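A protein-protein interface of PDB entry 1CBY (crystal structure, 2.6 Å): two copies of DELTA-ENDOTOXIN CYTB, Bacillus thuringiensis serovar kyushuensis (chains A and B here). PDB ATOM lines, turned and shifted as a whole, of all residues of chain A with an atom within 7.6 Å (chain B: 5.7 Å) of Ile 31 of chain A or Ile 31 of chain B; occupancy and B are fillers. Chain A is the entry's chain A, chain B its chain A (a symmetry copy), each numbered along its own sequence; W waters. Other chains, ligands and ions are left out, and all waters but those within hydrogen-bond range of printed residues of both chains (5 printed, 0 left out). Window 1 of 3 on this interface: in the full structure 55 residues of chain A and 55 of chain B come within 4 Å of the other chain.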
ATOM      1  N   PHE A  28      14.795 -25.860  16.470  1.00  0.00           N
ATOM      2  CA  PHE A  28      16.048 -25.551  17.143  1.00  0.00           C
ATOM      3  C   PHE A  28      15.766 -25.668  18.628  1.00  0.00           C
ATOM      4  O   PHE A  28      14.650 -25.404  19.070  1.00  0.00           O
ATOM      5  CB  PHE A  28      16.474 -24.107  16.865  1.00  0.00           C
ATOM      6  CG  PHE A  28      17.151 -23.909  15.547  1.00  0.00           C
ATOM      7  CD1 PHE A  28      16.413 -23.649  14.402  1.00  0.00           C
ATOM      8  CD2 PHE A  28      18.538 -23.957  15.456  1.00  0.00           C
ATOM      9  CE1 PHE A  28      17.044 -23.436  13.184  1.00  0.00           C
ATOM     10  CE2 PHE A  28      19.181 -23.746  14.245  1.00  0.00           C
ATOM     11  CZ  PHE A  28      18.432 -23.485  13.104  1.00  0.00           C
ATOM     12  N   LYS A  29      16.755 -26.107  19.390  1.00  0.00           N
ATOM     13  CA  LYS A  29      16.594 -26.202  20.830  1.00  0.00           C
ATOM     14  C   LYS A  29      17.163 -24.919  21.414  1.00  0.00           C
ATOM     15  O   LYS A  29      18.166 -24.397  20.923  1.00  0.00           O
ATOM     16  CB  LYS A  29      17.345 -27.411  21.390  1.00  0.00           C
ATOM     17  CG  LYS A  29      16.706 -28.736  21.043  1.00  0.00           C
ATOM     18  CD  LYS A  29      17.353 -29.876  21.800  1.00  0.00           C
ATOM     19  CE  LYS A  29      16.553 -31.161  21.642  1.00  0.00           C
ATOM     20  NZ  LYS A  29      15.144 -30.984  22.102  1.00  0.00           N
ATOM     21  N   HIS A  30      16.470 -24.365  22.397  1.00  0.00           N
ATOM     22  CA  HIS A  30      16.919 -23.153  23.063  1.00  0.00           C
ATOM     23  C   HIS A  30      17.092 -23.532  24.524  1.00  0.00           C
ATOM     24  O   HIS A  30      16.129 -23.548  25.291  1.00  0.00           O
ATOM     25  CB  HIS A  30      15.878 -22.051  22.924  1.00  0.00           C
ATOM     26  CG  HIS A  30      16.360 -20.715  23.386  1.00  0.00           C
ATOM     27  ND1 HIS A  30      15.988 -20.199  24.602  1.00  0.00           N
ATOM     28  CD2 HIS A  30      17.188 -19.845  22.759  1.00  0.00           C
ATOM     29  CE1 HIS A  30      16.592 -19.029  24.690  1.00  0.00           C
ATOM     30  NE2 HIS A  30      17.329 -18.772  23.599  1.00  0.00           N
ATOM     31  N   ILE A  31      18.319 -23.884  24.889  1.00  0.00           N
ATOM     32  CA  ILE A  31      18.630 -24.320  26.245  1.00  0.00           C
ATOM     33  C   ILE A  31      19.562 -23.384  27.003  1.00  0.00           C
ATOM     34  O   ILE A  31      20.690 -23.148  26.576  1.00  0.00           O
ATOM     35  CB  ILE A  31      19.321 -25.705  26.222  1.00  0.00           C
ATOM     36  CG1 ILE A  31      18.491 -26.706  25.421  1.00  0.00           C
ATOM     37  CG2 ILE A  31      19.539 -26.211  27.643  1.00  0.00           C
ATOM     38  CD1 ILE A  31      19.221 -27.998  25.137  1.00  0.00           C
ATOM     39  N   VAL A  32      19.092 -22.839  28.118  1.00  0.00           N
ATOM     40  CA  VAL A  32      19.947 -21.992  28.940  1.00  0.00           C
ATOM     41  C   VAL A  32      20.600 -22.994  29.885  1.00  0.00           C
ATOM     42  O   VAL A  32      19.940 -23.575  30.748  1.00  0.00           O
ATOM     43  CB  VAL A  32      19.152 -20.956  29.747  1.00  0.00           C
ATOM     44  CG1 VAL A  32      20.110 -20.034  30.485  1.00  0.00           C
ATOM     45  CG2 VAL A  32      18.261 -20.154  28.827  1.00  0.00           C
ATOM     46  N   LEU A  33      21.875 -23.262  29.644  1.00  0.00           N
ATOM     47  CA  LEU A  33      22.636 -24.219  30.429  1.00  0.00           C
ATOM     48  C   LEU A  33      23.485 -23.590  31.522  1.00  0.00           C
ATOM     49  O   LEU A  33      24.336 -22.735  31.251  1.00  0.00           O
ATOM     50  CB  LEU A  33      23.571 -25.013  29.515  1.00  0.00           C
ATOM     51  CG  LEU A  33      23.466 -26.536  29.453  1.00  0.00           C
ATOM     52  CD1 LEU A  33      24.718 -27.062  28.771  1.00  0.00           C
ATOM     53  CD2 LEU A  33      23.329 -27.142  30.839  1.00  0.00           C
ATOM     54  N   THR A  34      23.255 -24.026  32.753  1.00  0.00           N
ATOM     55  CA  THR A  34      24.040 -23.571  33.887  1.00  0.00           C
ATOM     56  C   THR A  34      24.545 -24.882  34.471  1.00  0.00           C
ATOM     57  O   THR A  34      23.785 -25.656  35.053  1.00  0.00           O
ATOM     58  CB  THR A  34      23.206 -22.793  34.902  1.00  0.00           C
ATOM     59  OG1 THR A  34      22.504 -21.741  34.228  1.00  0.00           O
ATOM     60  CG2 THR A  34      24.115 -22.172  35.953  1.00  0.00           C
ATOM     61  N   VAL A  35      25.814 -25.161  34.216  1.00  0.00           N
ATOM     62  CA  VAL A  35      26.445 -26.392  34.660  1.00  0.00           C
ATOM     63  C   VAL A  35      27.747 -26.046  35.397  1.00  0.00           C
ATOM     64  O   VAL A  35      28.440 -25.102  35.014  1.00  0.00           O
ATOM     65  CB  VAL A  35      26.739 -27.287  33.423  1.00  0.00           C
ATOM     66  CG1 VAL A  35      27.827 -26.677  32.557  1.00  0.00           C
ATOM     67  CG2 VAL A  35      27.121 -28.657  33.841  1.00  0.00           C
ATOM     68  N   ASP A  41      35.118 -19.241  35.158  1.00  0.00           N
ATOM     69  CA  ASP A  41      34.367 -18.780  33.991  1.00  0.00           C
ATOM     70  C   ASP A  41      33.733 -17.416  34.265  1.00  0.00           C
ATOM     71  O   ASP A  41      32.762 -17.312  35.010  1.00  0.00           O
ATOM     72  CB  ASP A  41      33.273 -19.798  33.639  1.00  0.00           C
ATOM     73  CG  ASP A  41      32.669 -19.574  32.253  1.00  0.00           C
ATOM     74  OD1 ASP A  41      32.681 -18.433  31.744  1.00  0.00           O
ATOM     75  OD2 ASP A  41      32.169 -20.556  31.666  1.00  0.00           O
ATOM     76  N   PHE A  43      32.527 -15.382  31.741  1.00  0.00           N
ATOM     77  CA  PHE A  43      31.915 -15.029  30.466  1.00  0.00           C
ATOM     78  C   PHE A  43      30.459 -15.449  30.403  1.00  0.00           C
ATOM     79  O   PHE A  43      30.101 -16.531  30.870  1.00  0.00           O
ATOM     80  CB  PHE A  43      32.642 -15.731  29.307  1.00  0.00           C
ATOM     81  CG  PHE A  43      33.748 -14.927  28.696  1.00  0.00           C
ATOM     82  CD1 PHE A  43      33.484 -13.708  28.082  1.00  0.00           C
ATOM     83  CD2 PHE A  43      35.058 -15.391  28.726  1.00  0.00           C
ATOM     84  CE1 PHE A  43      34.511 -12.957  27.502  1.00  0.00           C
ATOM     85  CE2 PHE A  43      36.092 -14.649  28.150  1.00  0.00           C
ATOM     86  CZ  PHE A  43      35.817 -13.429  27.536  1.00  0.00           C
ATOM     87  N   ASN A  44      29.619 -14.562  29.879  1.00  0.00           N
ATOM     88  CA  ASN A  44      28.210 -14.874  29.665  1.00  0.00           C
ATOM     89  C   ASN A  44      28.306 -15.459  28.248  1.00  0.00           C
ATOM     90  O   ASN A  44      28.575 -14.745  27.272  1.00  0.00           O
ATOM     91  CB  ASN A  44      27.357 -13.605  29.680  1.00  0.00           C
ATOM     92  CG  ASN A  44      25.867 -13.892  29.848  1.00  0.00           C
ATOM     93  OD1 ASN A  44      25.077 -12.971  30.043  1.00  0.00           O
ATOM     94  ND2 ASN A  44      25.478 -15.161  29.779  1.00  0.00           N
ATOM     95  N   THR A  45      28.182 -16.773  28.161  1.00  0.00           N
ATOM     96  CA  THR A  45      28.328 -17.479  26.903  1.00  0.00           C
ATOM     97  C   THR A  45      27.060 -17.730  26.077  1.00  0.00           C
ATOM     98  O   THR A  45      26.020 -18.130  26.609  1.00  0.00           O
ATOM     99  CB  THR A  45      29.053 -18.799  27.163  1.00  0.00           C
ATOM    100  OG1 THR A  45      30.160 -18.556  28.040  1.00  0.00           O
ATOM    101  CG2 THR A  45      29.584 -19.376  25.883  1.00  0.00           C
ATOM    102  N   VAL A  46      27.164 -17.482  24.772  1.00  0.00           N
ATOM    103  CA  VAL A  46      26.067 -17.694  23.830  1.00  0.00           C
ATOM    104  C   VAL A  46      26.619 -18.541  22.686  1.00  0.00           C
ATOM    105  O   VAL A  46      27.546 -18.125  21.987  1.00  0.00           O
ATOM    106  CB  VAL A  46      25.514 -16.354  23.278  1.00  0.00           C
ATOM    107  CG1 VAL A  46      24.472 -16.608  22.201  1.00  0.00           C
ATOM    108  CG2 VAL A  46      24.892 -15.543  24.399  1.00  0.00           C
ATOM    109  N   PHE A  47      26.074 -19.747  22.532  1.00  0.00           N
ATOM    110  CA  PHE A  47      26.499 -20.691  21.496  1.00  0.00           C
ATOM    111  C   PHE A  47      25.416 -20.973  20.461  1.00  0.00           C
ATOM    112  O   PHE A  47      24.325 -21.434  20.806  1.00  0.00           O
ATOM    113  CB  PHE A  47      26.880 -22.043  22.120  1.00  0.00           C
ATOM    114  CG  PHE A  47      28.262 -22.096  22.724  1.00  0.00           C
ATOM    115  CD1 PHE A  47      29.088 -20.982  22.746  1.00  0.00           C
ATOM    116  CD2 PHE A  47      28.733 -23.286  23.277  1.00  0.00           C
ATOM    117  CE1 PHE A  47      30.357 -21.051  23.306  1.00  0.00           C
ATOM    118  CE2 PHE A  47      29.998 -23.363  23.838  1.00  0.00           C
ATOM    119  CZ  PHE A  47      30.811 -22.245  23.853  1.00  0.00           C
ATOM    120  N   TYR A  48      25.734 -20.727  19.195  1.00  0.00           N
ATOM    121  CA  TYR A  48      24.825 -21.010  18.084  1.00  0.00           C
ATOM    122  C   TYR A  48      25.670 -21.903  17.181  1.00  0.00           C
ATOM    123  O   TYR A  48      26.330 -21.425  16.255  1.00  0.00           O
ATOM    124  CB  TYR A  48      24.423 -19.724  17.350  1.00  0.00           C
ATOM    125  CG  TYR A  48      23.383 -19.940  16.266  1.00  0.00           C
ATOM    126  CD1 TYR A  48      23.746 -20.413  15.005  1.00  0.00           C
ATOM    127  CD2 TYR A  48      22.036 -19.683  16.504  1.00  0.00           C
ATOM    128  CE1 TYR A  48      22.798 -20.625  14.009  1.00  0.00           C
ATOM    129  CE2 TYR A  48      21.076 -19.893  15.513  1.00  0.00           C
ATOM    130  CZ  TYR A  48      21.466 -20.363  14.267  1.00  0.00           C
ATOM    131  OH  TYR A  48      20.527 -20.572  13.280  1.00  0.00           O
ATOM    132  N   ILE A  54      30.391 -28.363  19.439  1.00  0.00           N
ATOM    133  CA  ILE A  54      30.269 -27.780  20.768  1.00  0.00           C
ATOM    134  C   ILE A  54      31.615 -27.844  21.483  1.00  0.00           C
ATOM    135  O   ILE A  54      32.034 -26.875  22.117  1.00  0.00           O
ATOM    136  CB  ILE A  54      29.163 -28.494  21.597  1.00  0.00           C
ATOM    137  CG1 ILE A  54      27.779 -28.093  21.065  1.00  0.00           C
ATOM    138  CG2 ILE A  54      29.306 -28.177  23.085  1.00  0.00           C
ATOM    139  CD1 ILE A  54      26.620 -28.847  21.679  1.00  0.00           C
ATOM    140  N   LEU A  58      33.636 -24.727  23.011  1.00  0.00           N
ATOM    141  CA  LEU A  58      33.973 -24.716  24.425  1.00  0.00           C
ATOM    142  C   LEU A  58      35.472 -24.491  24.614  1.00  0.00           C
ATOM    143  O   LEU A  58      35.892 -23.767  25.523  1.00  0.00           O
ATOM    144  CB  LEU A  58      33.519 -26.026  25.070  1.00  0.00           C
ATOM    145  CG  LEU A  58      32.970 -25.963  26.497  1.00  0.00           C
ATOM    146  CD1 LEU A  58      32.091 -24.734  26.699  1.00  0.00           C
ATOM    147  CD2 LEU A  58      32.187 -27.229  26.780  1.00  0.00           C
ATOM    148  N   ALA A  61      36.178 -20.877  23.873  1.00  0.00           N
ATOM    149  CA  ALA A  61      35.645 -20.073  24.965  1.00  0.00           C
ATOM    150  C   ALA A  61      36.628 -20.055  26.143  1.00  0.00           C
ATOM    151  O   ALA A  61      37.038 -18.985  26.604  1.00  0.00           O
ATOM    152  CB  ALA A  61      34.297 -20.622  25.409  1.00  0.00           C
ATOM    153  N   TRP A 154      30.142 -12.873  35.285  1.00  0.00           N
ATOM    154  CA  TRP A 154      30.360 -12.037  34.105  1.00  0.00           C
ATOM    155  C   TRP A 154      30.238 -10.537  34.337  1.00  0.00           C
ATOM    156  O   TRP A 154      30.517  -9.747  33.433  1.00  0.00           O
ATOM    157  CB  TRP A 154      29.464 -12.477  32.939  1.00  0.00           C
ATOM    158  CG  TRP A 154      27.998 -12.410  33.208  1.00  0.00           C
ATOM    159  CD1 TRP A 154      27.199 -11.313  33.108  1.00  0.00           C
ATOM    160  CD2 TRP A 154      27.149 -13.490  33.609  1.00  0.00           C
ATOM    161  NE1 TRP A 154      25.902 -11.642  33.421  1.00  0.00           N
ATOM    162  CE2 TRP A 154      25.844 -12.973  33.733  1.00  0.00           C
ATOM    163  CE3 TRP A 154      27.366 -14.848  33.872  1.00  0.00           C
ATOM    164  CZ2 TRP A 154      24.759 -13.762  34.108  1.00  0.00           C
ATOM    165  CZ3 TRP A 154      26.286 -15.635  34.243  1.00  0.00           C
ATOM    166  CH2 TRP A 154      24.998 -15.087  34.360  1.00  0.00           C
ATOM    167  N   LEU A 172      30.607 -13.738  25.389  1.00  0.00           N
ATOM    168  CA  LEU A 172      31.339 -14.492  24.380  1.00  0.00           C
ATOM    169  C   LEU A 172      30.341 -15.155  23.458  1.00  0.00           C
ATOM    170  O   LEU A 172      29.485 -15.924  23.902  1.00  0.00           O
ATOM    171  CB  LEU A 172      32.260 -15.552  24.994  1.00  0.00           C
ATOM    172  CG  LEU A 172      33.082 -16.308  23.938  1.00  0.00           C
ATOM    173  CD1 LEU A 172      34.568 -16.215  24.227  1.00  0.00           C
ATOM    174  CD2 LEU A 172      32.635 -17.761  23.844  1.00  0.00           C
ATOM    175  N   PHE A 237      33.107 -31.330  29.250  1.00  0.00           N
ATOM    176  CA  PHE A 237      33.036 -30.353  30.329  1.00  0.00           C
ATOM    177  C   PHE A 237      34.137 -30.452  31.385  1.00  0.00           C
ATOM    178  O   PHE A 237      34.181 -29.645  32.312  1.00  0.00           O
ATOM    179  CB  PHE A 237      31.645 -30.364  30.962  1.00  0.00           C
ATOM    180  CG  PHE A 237      30.568 -29.854  30.044  1.00  0.00           C
ATOM    181  CD1 PHE A 237      29.912 -30.714  29.169  1.00  0.00           C
ATOM    182  CD2 PHE A 237      30.238 -28.503  30.022  1.00  0.00           C
ATOM    183  CE1 PHE A 237      28.945 -30.235  28.284  1.00  0.00           C
ATOM    184  CE2 PHE A 237      29.272 -28.017  29.140  1.00  0.00           C
ATOM    185  CZ  PHE A 237      28.627 -28.884  28.271  1.00  0.00           C
ATOM    186  N   LYS B  29      29.237 -22.492  34.417  1.00  0.00           N
ATOM    187  CA  LYS B  29      29.198 -22.008  33.049  1.00  0.00           C
ATOM    188  C   LYS B  29      27.761 -21.592  32.777  1.00  0.00           C
ATOM    189  O   LYS B  29      26.823 -22.240  33.246  1.00  0.00           O
ATOM    190  CB  LYS B  29      29.623 -23.100  32.066  1.00  0.00           C
ATOM    191  CG  LYS B  29      31.102 -23.415  32.111  1.00  0.00           C
ATOM    192  CD  LYS B  29      31.505 -24.331  30.976  1.00  0.00           C
ATOM    193  CE  LYS B  29      33.019 -24.444  30.876  1.00  0.00           C
ATOM    194  NZ  LYS B  29      33.654 -23.105  30.695  1.00  0.00           N
ATOM    195  N   HIS B  30      27.595 -20.464  32.104  1.00  0.00           N
ATOM    196  CA  HIS B  30      26.273 -19.970  31.752  1.00  0.00           C
ATOM    197  C   HIS B  30      26.257 -19.898  30.235  1.00  0.00           C
ATOM    198  O   HIS B  30      26.734 -18.928  29.642  1.00  0.00           O
ATOM    199  CB  HIS B  30      26.046 -18.589  32.347  1.00  0.00           C
ATOM    200  CG  HIS B  30      24.636 -18.111  32.220  1.00  0.00           C
ATOM    201  ND1 HIS B  30      24.274 -17.190  31.268  1.00  0.00           N
ATOM    202  CD2 HIS B  30      23.546 -18.468  32.940  1.00  0.00           C
ATOM    203  CE1 HIS B  30      22.978 -17.004  31.428  1.00  0.00           C
ATOM    204  NE2 HIS B  30      22.493 -17.757  32.428  1.00  0.00           N
ATOM    205  N   ILE B  31      25.751 -20.955  29.610  1.00  0.00           N
ATOM    206  CA  ILE B  31      25.711 -21.052  28.156  1.00  0.00           C
ATOM    207  C   ILE B  31      24.307 -21.063  27.569  1.00  0.00           C
ATOM    208  O   ILE B  31      23.510 -21.946  27.876  1.00  0.00           O
ATOM    209  CB  ILE B  31      26.396 -22.358  27.684  1.00  0.00           C
ATOM    210  CG1 ILE B  31      27.798 -22.474  28.279  1.00  0.00           C
ATOM    211  CG2 ILE B  31      26.460 -22.401  26.162  1.00  0.00           C
ATOM    212  CD1 ILE B  31      28.423 -23.835  28.076  1.00  0.00           C
ATOM    213  N   VAL B  32      23.995 -20.078  26.735  1.00  0.00           N
ATOM    214  CA  VAL B  32      22.697 -20.059  26.072  1.00  0.00           C
ATOM    215  C   VAL B  32      22.962 -20.852  24.797  1.00  0.00           C
ATOM    216  O   VAL B  32      23.688 -20.401  23.909  1.00  0.00           O
ATOM    217  CB  VAL B  32      22.236 -18.637  25.717  1.00  0.00           C
ATOM    218  CG1 VAL B  32      20.831 -18.682  25.140  1.00  0.00           C
ATOM    219  CG2 VAL B  32      22.269 -17.759  26.946  1.00  0.00           C
ATOM    220  N   LEU B  33      22.448 -22.072  24.764  1.00  0.00           N
ATOM    221  CA  LEU B  33      22.636 -22.971  23.637  1.00  0.00           C
ATOM    222  C   LEU B  33      21.473 -22.987  22.658  1.00  0.00           C
ATOM    223  O   LEU B  33      20.330 -23.270  23.034  1.00  0.00           O
ATOM    224  CB  LEU B  33      22.836 -24.399  24.142  1.00  0.00           C
ATOM    225  CG  LEU B  33      24.111 -25.163  23.783  1.00  0.00           C
ATOM    226  CD1 LEU B  33      23.877 -26.633  24.099  1.00  0.00           C
ATOM    227  CD2 LEU B  33      24.469 -24.992  22.318  1.00  0.00           C
ATOM    228  N   THR B  34      21.775 -22.694  21.400  1.00  0.00           N
ATOM    229  CA  THR B  34      20.784 -22.743  20.341  1.00  0.00           C
ATOM    230  C   THR B  34      21.432 -23.689  19.342  1.00  0.00           C
ATOM    231  O   THR B  34      22.412 -23.346  18.680  1.00  0.00           O
ATOM    232  CB  THR B  34      20.520 -21.373  19.721  1.00  0.00           C
ATOM    233  OG1 THR B  34      20.206 -20.438  20.760  1.00  0.00           O
ATOM    234  CG2 THR B  34      19.335 -21.454  18.769  1.00  0.00           C
ATOM    235  N   VAL B  35      20.933 -24.916  19.319  1.00  0.00           N
ATOM    236  CA  VAL B  35      21.463 -25.957  18.458  1.00  0.00           C
ATOM    237  C   VAL B  35      20.306 -26.588  17.668  1.00  0.00           C
ATOM    238  O   VAL B  35      19.204 -26.729  18.199  1.00  0.00           O
ATOM    239  CB  VAL B  35      22.174 -27.028  19.332  1.00  0.00           C
ATOM    240  CG1 VAL B  35      21.169 -27.802  20.169  1.00  0.00           C
ATOM    241  CG2 VAL B  35      22.967 -27.957  18.492  1.00  0.00           C
ATOM    242  N   THR B  45      13.779 -23.939  27.097  1.00  0.00           N
ATOM    243  CA  THR B  45      14.431 -24.795  28.068  1.00  0.00           C
ATOM    244  C   THR B  45      15.506 -24.166  28.963  1.00  0.00           C
ATOM    245  O   THR B  45      16.365 -23.412  28.497  1.00  0.00           O
ATOM    246  CB  THR B  45      15.003 -26.012  27.340  1.00  0.00           C
ATOM    247  OG1 THR B  45      14.023 -26.504  26.418  1.00  0.00           O
ATOM    248  CG2 THR B  45      15.327 -27.110  28.313  1.00  0.00           C
ATOM    249  N   VAL B  46      15.437 -24.484  30.256  1.00  0.00           N
ATOM    250  CA  VAL B  46      16.396 -24.001  31.247  1.00  0.00           C
ATOM    251  C   VAL B  46      16.902 -25.223  32.011  1.00  0.00           C
ATOM    252  O   VAL B  46      16.121 -25.927  32.657  1.00  0.00           O
ATOM    253  CB  VAL B  46      15.749 -22.992  32.231  1.00  0.00           C
ATOM    254  CG1 VAL B  46      16.727 -22.614  33.332  1.00  0.00           C
ATOM    255  CG2 VAL B  46      15.316 -21.741  31.490  1.00  0.00           C
ATOM    256  N   PHE B  47      18.201 -25.493  31.893  1.00  0.00           N
ATOM    257  CA  PHE B  47      18.842 -26.636  32.545  1.00  0.00           C
ATOM    258  C   PHE B  47      19.861 -26.229  33.603  1.00  0.00           C
ATOM    259  O   PHE B  47      20.826 -25.521  33.304  1.00  0.00           O
ATOM    260  CB  PHE B  47      19.592 -27.496  31.515  1.00  0.00           C
ATOM    261  CG  PHE B  47      18.721 -28.445  30.726  1.00  0.00           C
ATOM    262  CD1 PHE B  47      17.346 -28.483  30.902  1.00  0.00           C
ATOM    263  CD2 PHE B  47      19.299 -29.307  29.796  1.00  0.00           C
ATOM    264  CE1 PHE B  47      16.563 -29.364  30.167  1.00  0.00           C
ATOM    265  CE2 PHE B  47      18.524 -30.188  29.058  1.00  0.00           C
ATOM    266  CZ  PHE B  47      17.155 -30.217  29.244  1.00  0.00           C
ATOM    267  N   LEU B  58      17.551 -34.036  28.927  1.00  0.00           N
ATOM    268  CA  LEU B  58      17.136 -33.894  27.541  1.00  0.00           C
ATOM    269  C   LEU B  58      16.036 -34.902  27.207  1.00  0.00           C
ATOM    270  O   LEU B  58      15.083 -34.581  26.491  1.00  0.00           O
ATOM    271  CB  LEU B  58      18.347 -34.066  26.623  1.00  0.00           C
ATOM    272  CG  LEU B  58      18.418 -33.193  25.368  1.00  0.00           C
ATOM    273  CD1 LEU B  58      17.942 -31.773  25.654  1.00  0.00           C
ATOM    274  CD2 LEU B  58      19.843 -33.184  24.854  1.00  0.00           C
ATOM    275  N   PHE B 237      22.171 -35.441  21.214  1.00  0.00           N
ATOM    276  CA  PHE B 237      21.287 -34.547  20.480  1.00  0.00           C
ATOM    277  C   PHE B 237      20.554 -35.169  19.291  1.00  0.00           C
ATOM    278  O   PHE B 237      19.757 -34.501  18.636  1.00  0.00           O
ATOM    279  CB  PHE B 237      22.033 -33.275  20.079  1.00  0.00           C
ATOM    280  CG  PHE B 237      22.406 -32.408  21.250  1.00  0.00           C
ATOM    281  CD1 PHE B 237      23.603 -32.606  21.930  1.00  0.00           C
ATOM    282  CD2 PHE B 237      21.540 -31.417  21.702  1.00  0.00           C
ATOM    283  CE1 PHE B 237      23.931 -31.834  23.045  1.00  0.00           C
ATOM    284  CE2 PHE B 237      21.861 -30.641  22.817  1.00  0.00           C
ATOM    285  CZ  PHE B 237      23.055 -30.851  23.488  1.00  0.00           C
HETATM  286  O   HOH W   1      20.096 -22.537  33.632  1.00  0.00           O
HETATM  287  O   HOH W   2      34.085 -20.922  28.882  1.00  0.00           O
HETATM  288  O   HOH W   3      22.358 -19.140  21.449  1.00  0.00           O
HETATM  289  O   HOH W   4      14.411 -25.614  23.611  1.00  0.00           O
HETATM  290  O   HOH W   5      29.633 -19.174  30.898  1.00  0.00           O
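The backbone carbonyl oxygen of Phe 43 of chain A lies within hydrogen-bond range of the side-chain hydroxyl of Thr 45 of chain A.
The backbone carbonyl oxygen (O) of Asn 44 of chain A sits at hydrogen-bond distance from the backbone NH (N) of Leu 172 of chain A.
N of Phe 43 of chain A sits at hydrogen-bond distance from OD1 of Asp 41 of chain A, 3.1 Å away.
CA of Phe 28 of chain A touches O of Val 35 of chain B, at 3.5 Å.
Leu 33 of chain A touches His 30 of chain B (O to CA, 3.4 Å).
Thr 34 of chain A touches His 30 of chain B (OG1 to CD2, 3.7 Å).
CD2 of Phe 47 of chain A touches CG2 of Ile 31 of chain B (3.8 Å).
Thr 34 of chain B touches Tyr 48 of chain A (O to CA, 3.4 Å).
Of the printed residues of chain B, Ile 31 of chain A touches Ile 31 (3.3 Å), Val 32 (3.7 Å), Leu 33 (2.7 Å), Thr 45 (3.3 Å) and Phe 47 (3.8 Å).
Printed residues of chain B within 4 Å of His 30 of chain A: Val 32, Leu 33, Thr 34 and Thr 45.
Of the printed residues of chain A, Lys 29 of chain B touches Leu 33, Thr 34, Val 35 and Asp 41.
The nearest printed residue of chain B that does not touch Ile 31 of chain A is Leu 58 of chain B (4.02 Å).
Water W3 lies within hydrogen-bond range of the side-chain hydroxyl of Thr 34 of chain B, the backbone carbonyl oxygen of Val 32 of chain B and the backbone carbonyl oxygen of Phe 47 of chain A.
Water W1 lies within hydrogen-bond range of OG1 of Thr 34 of chain A (2.6 Å), O of Val 32 of chain A (3.1 Å) and O of Phe 47 of chain B (3.1 Å).
Lys 29 of chain A touches Val 35 of chain B, and with the chains exchanged Val 35 of chain A touches Lys 29 of chain B.
Ile 31 of chain A touches Phe 47 of chain B, and with the chains exchanged Phe 47 of chain A touches Ile 31 of chain B.
Val 32 of chain A touches Phe 47 of chain B, and with the chains exchanged Phe 47 of chain A touches Val 32 of chain B.
Hydrophobic or aromatic side chains of chain A within 4 Å of the printed part of chain B: Phe 28, His 30, Ile 31, Val 32, Leu 33, Phe 47, Tyr 48 and Trp 154.
Of the 12 printed residues of chain B, 10 touch a printed residue of chain A.
Hydrophobic or aromatic side chains of chain B within 4 Å of the printed part of chain A: His 30, Ile 31, Val 32, Leu 33 and Phe 47.
Among the printed residues, 38 pairs touch across the chains.
Among the printed residues, Asp or Glu carboxylates within 4 Å of a Lys or Arg side-chain nitrogen of the other chain: Asp 41 of chain A with Lys 29 of chain B (3.1 Å).
O of Ile 31 of chain A is in hydrogen-bond range of N of Leu 33 of chain B (2.7 Å).
The backbone carbonyl oxygen of Lys 29 of chain A sits close to the backbone carbonyl oxygen of Leu 33 of chain B, at 3.2 Å.
The side-chain amino group (NZ) of Lys 29 of chain B is in salt-bridge range of the side-chain carboxylate (OD2) of Asp 41 of chain A (3.1 Å).
The backbone carbonyl oxygen (O) of Leu 33 of chain A lies close to the backbone carbonyl oxygen (O) of Lys 29 of chain B.
The backbone carbonyl oxygen (O) of His 30 of chain A sits at hydrogen-bond distance from the backbone NH (N) of Thr 45 of chain B, 3.0 Å away.
N of Val 32 of chain B is in hydrogen-bond range of O of Thr 45 of chain A (2.8 Å).
The backbone NH (N) of Lys 29 of chain A is in hydrogen-bond range of the backbone carbonyl oxygen (O) of Val 35 of chain B.
The side-chain amide nitrogen (ND2) of Asn 44 of chain A is in hydrogen-bond range of a ring nitrogen (ND1) of His 30 of chain B (2.8 Å).
The backbone carbonyl oxygen (O) of Ile 31 of chain A sits close to the backbone carbonyl oxygen (O) of Ile 31 of chain B.
N of Phe 47 of chain A is in hydrogen-bond range of O of Val 32 of chain B, 2.8 Å away.
The backbone NH (N) of Leu 33 of chain A sits at hydrogen-bond distance from the backbone carbonyl oxygen (O) of Ile 31 of chain B (2.7 Å).
N of Thr 45 of chain A lies within hydrogen-bond range of O of His 30 of chain B (3.0 Å).
O of Thr 45 of chain B lies within hydrogen-bond range of N of Val 32 of chain A (2.8 Å).
O of Phe 47 of chain A sits at hydrogen-bond distance from N of Thr 34 of chain B.
The backbone carbonyl oxygen of Phe 47 of chain B sits at hydrogen-bond distance from the backbone NH of Thr 34 of chain A (2.9 Å).
O of Val 32 of chain A is in hydrogen-bond range of N of Phe 47 of chain B, at 2.8 Å.
The backbone carbonyl oxygen (O) of Val 35 of chain A sits at hydrogen-bond distance from the backbone NH (N) of Lys 29 of chain B (2.8 Å).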
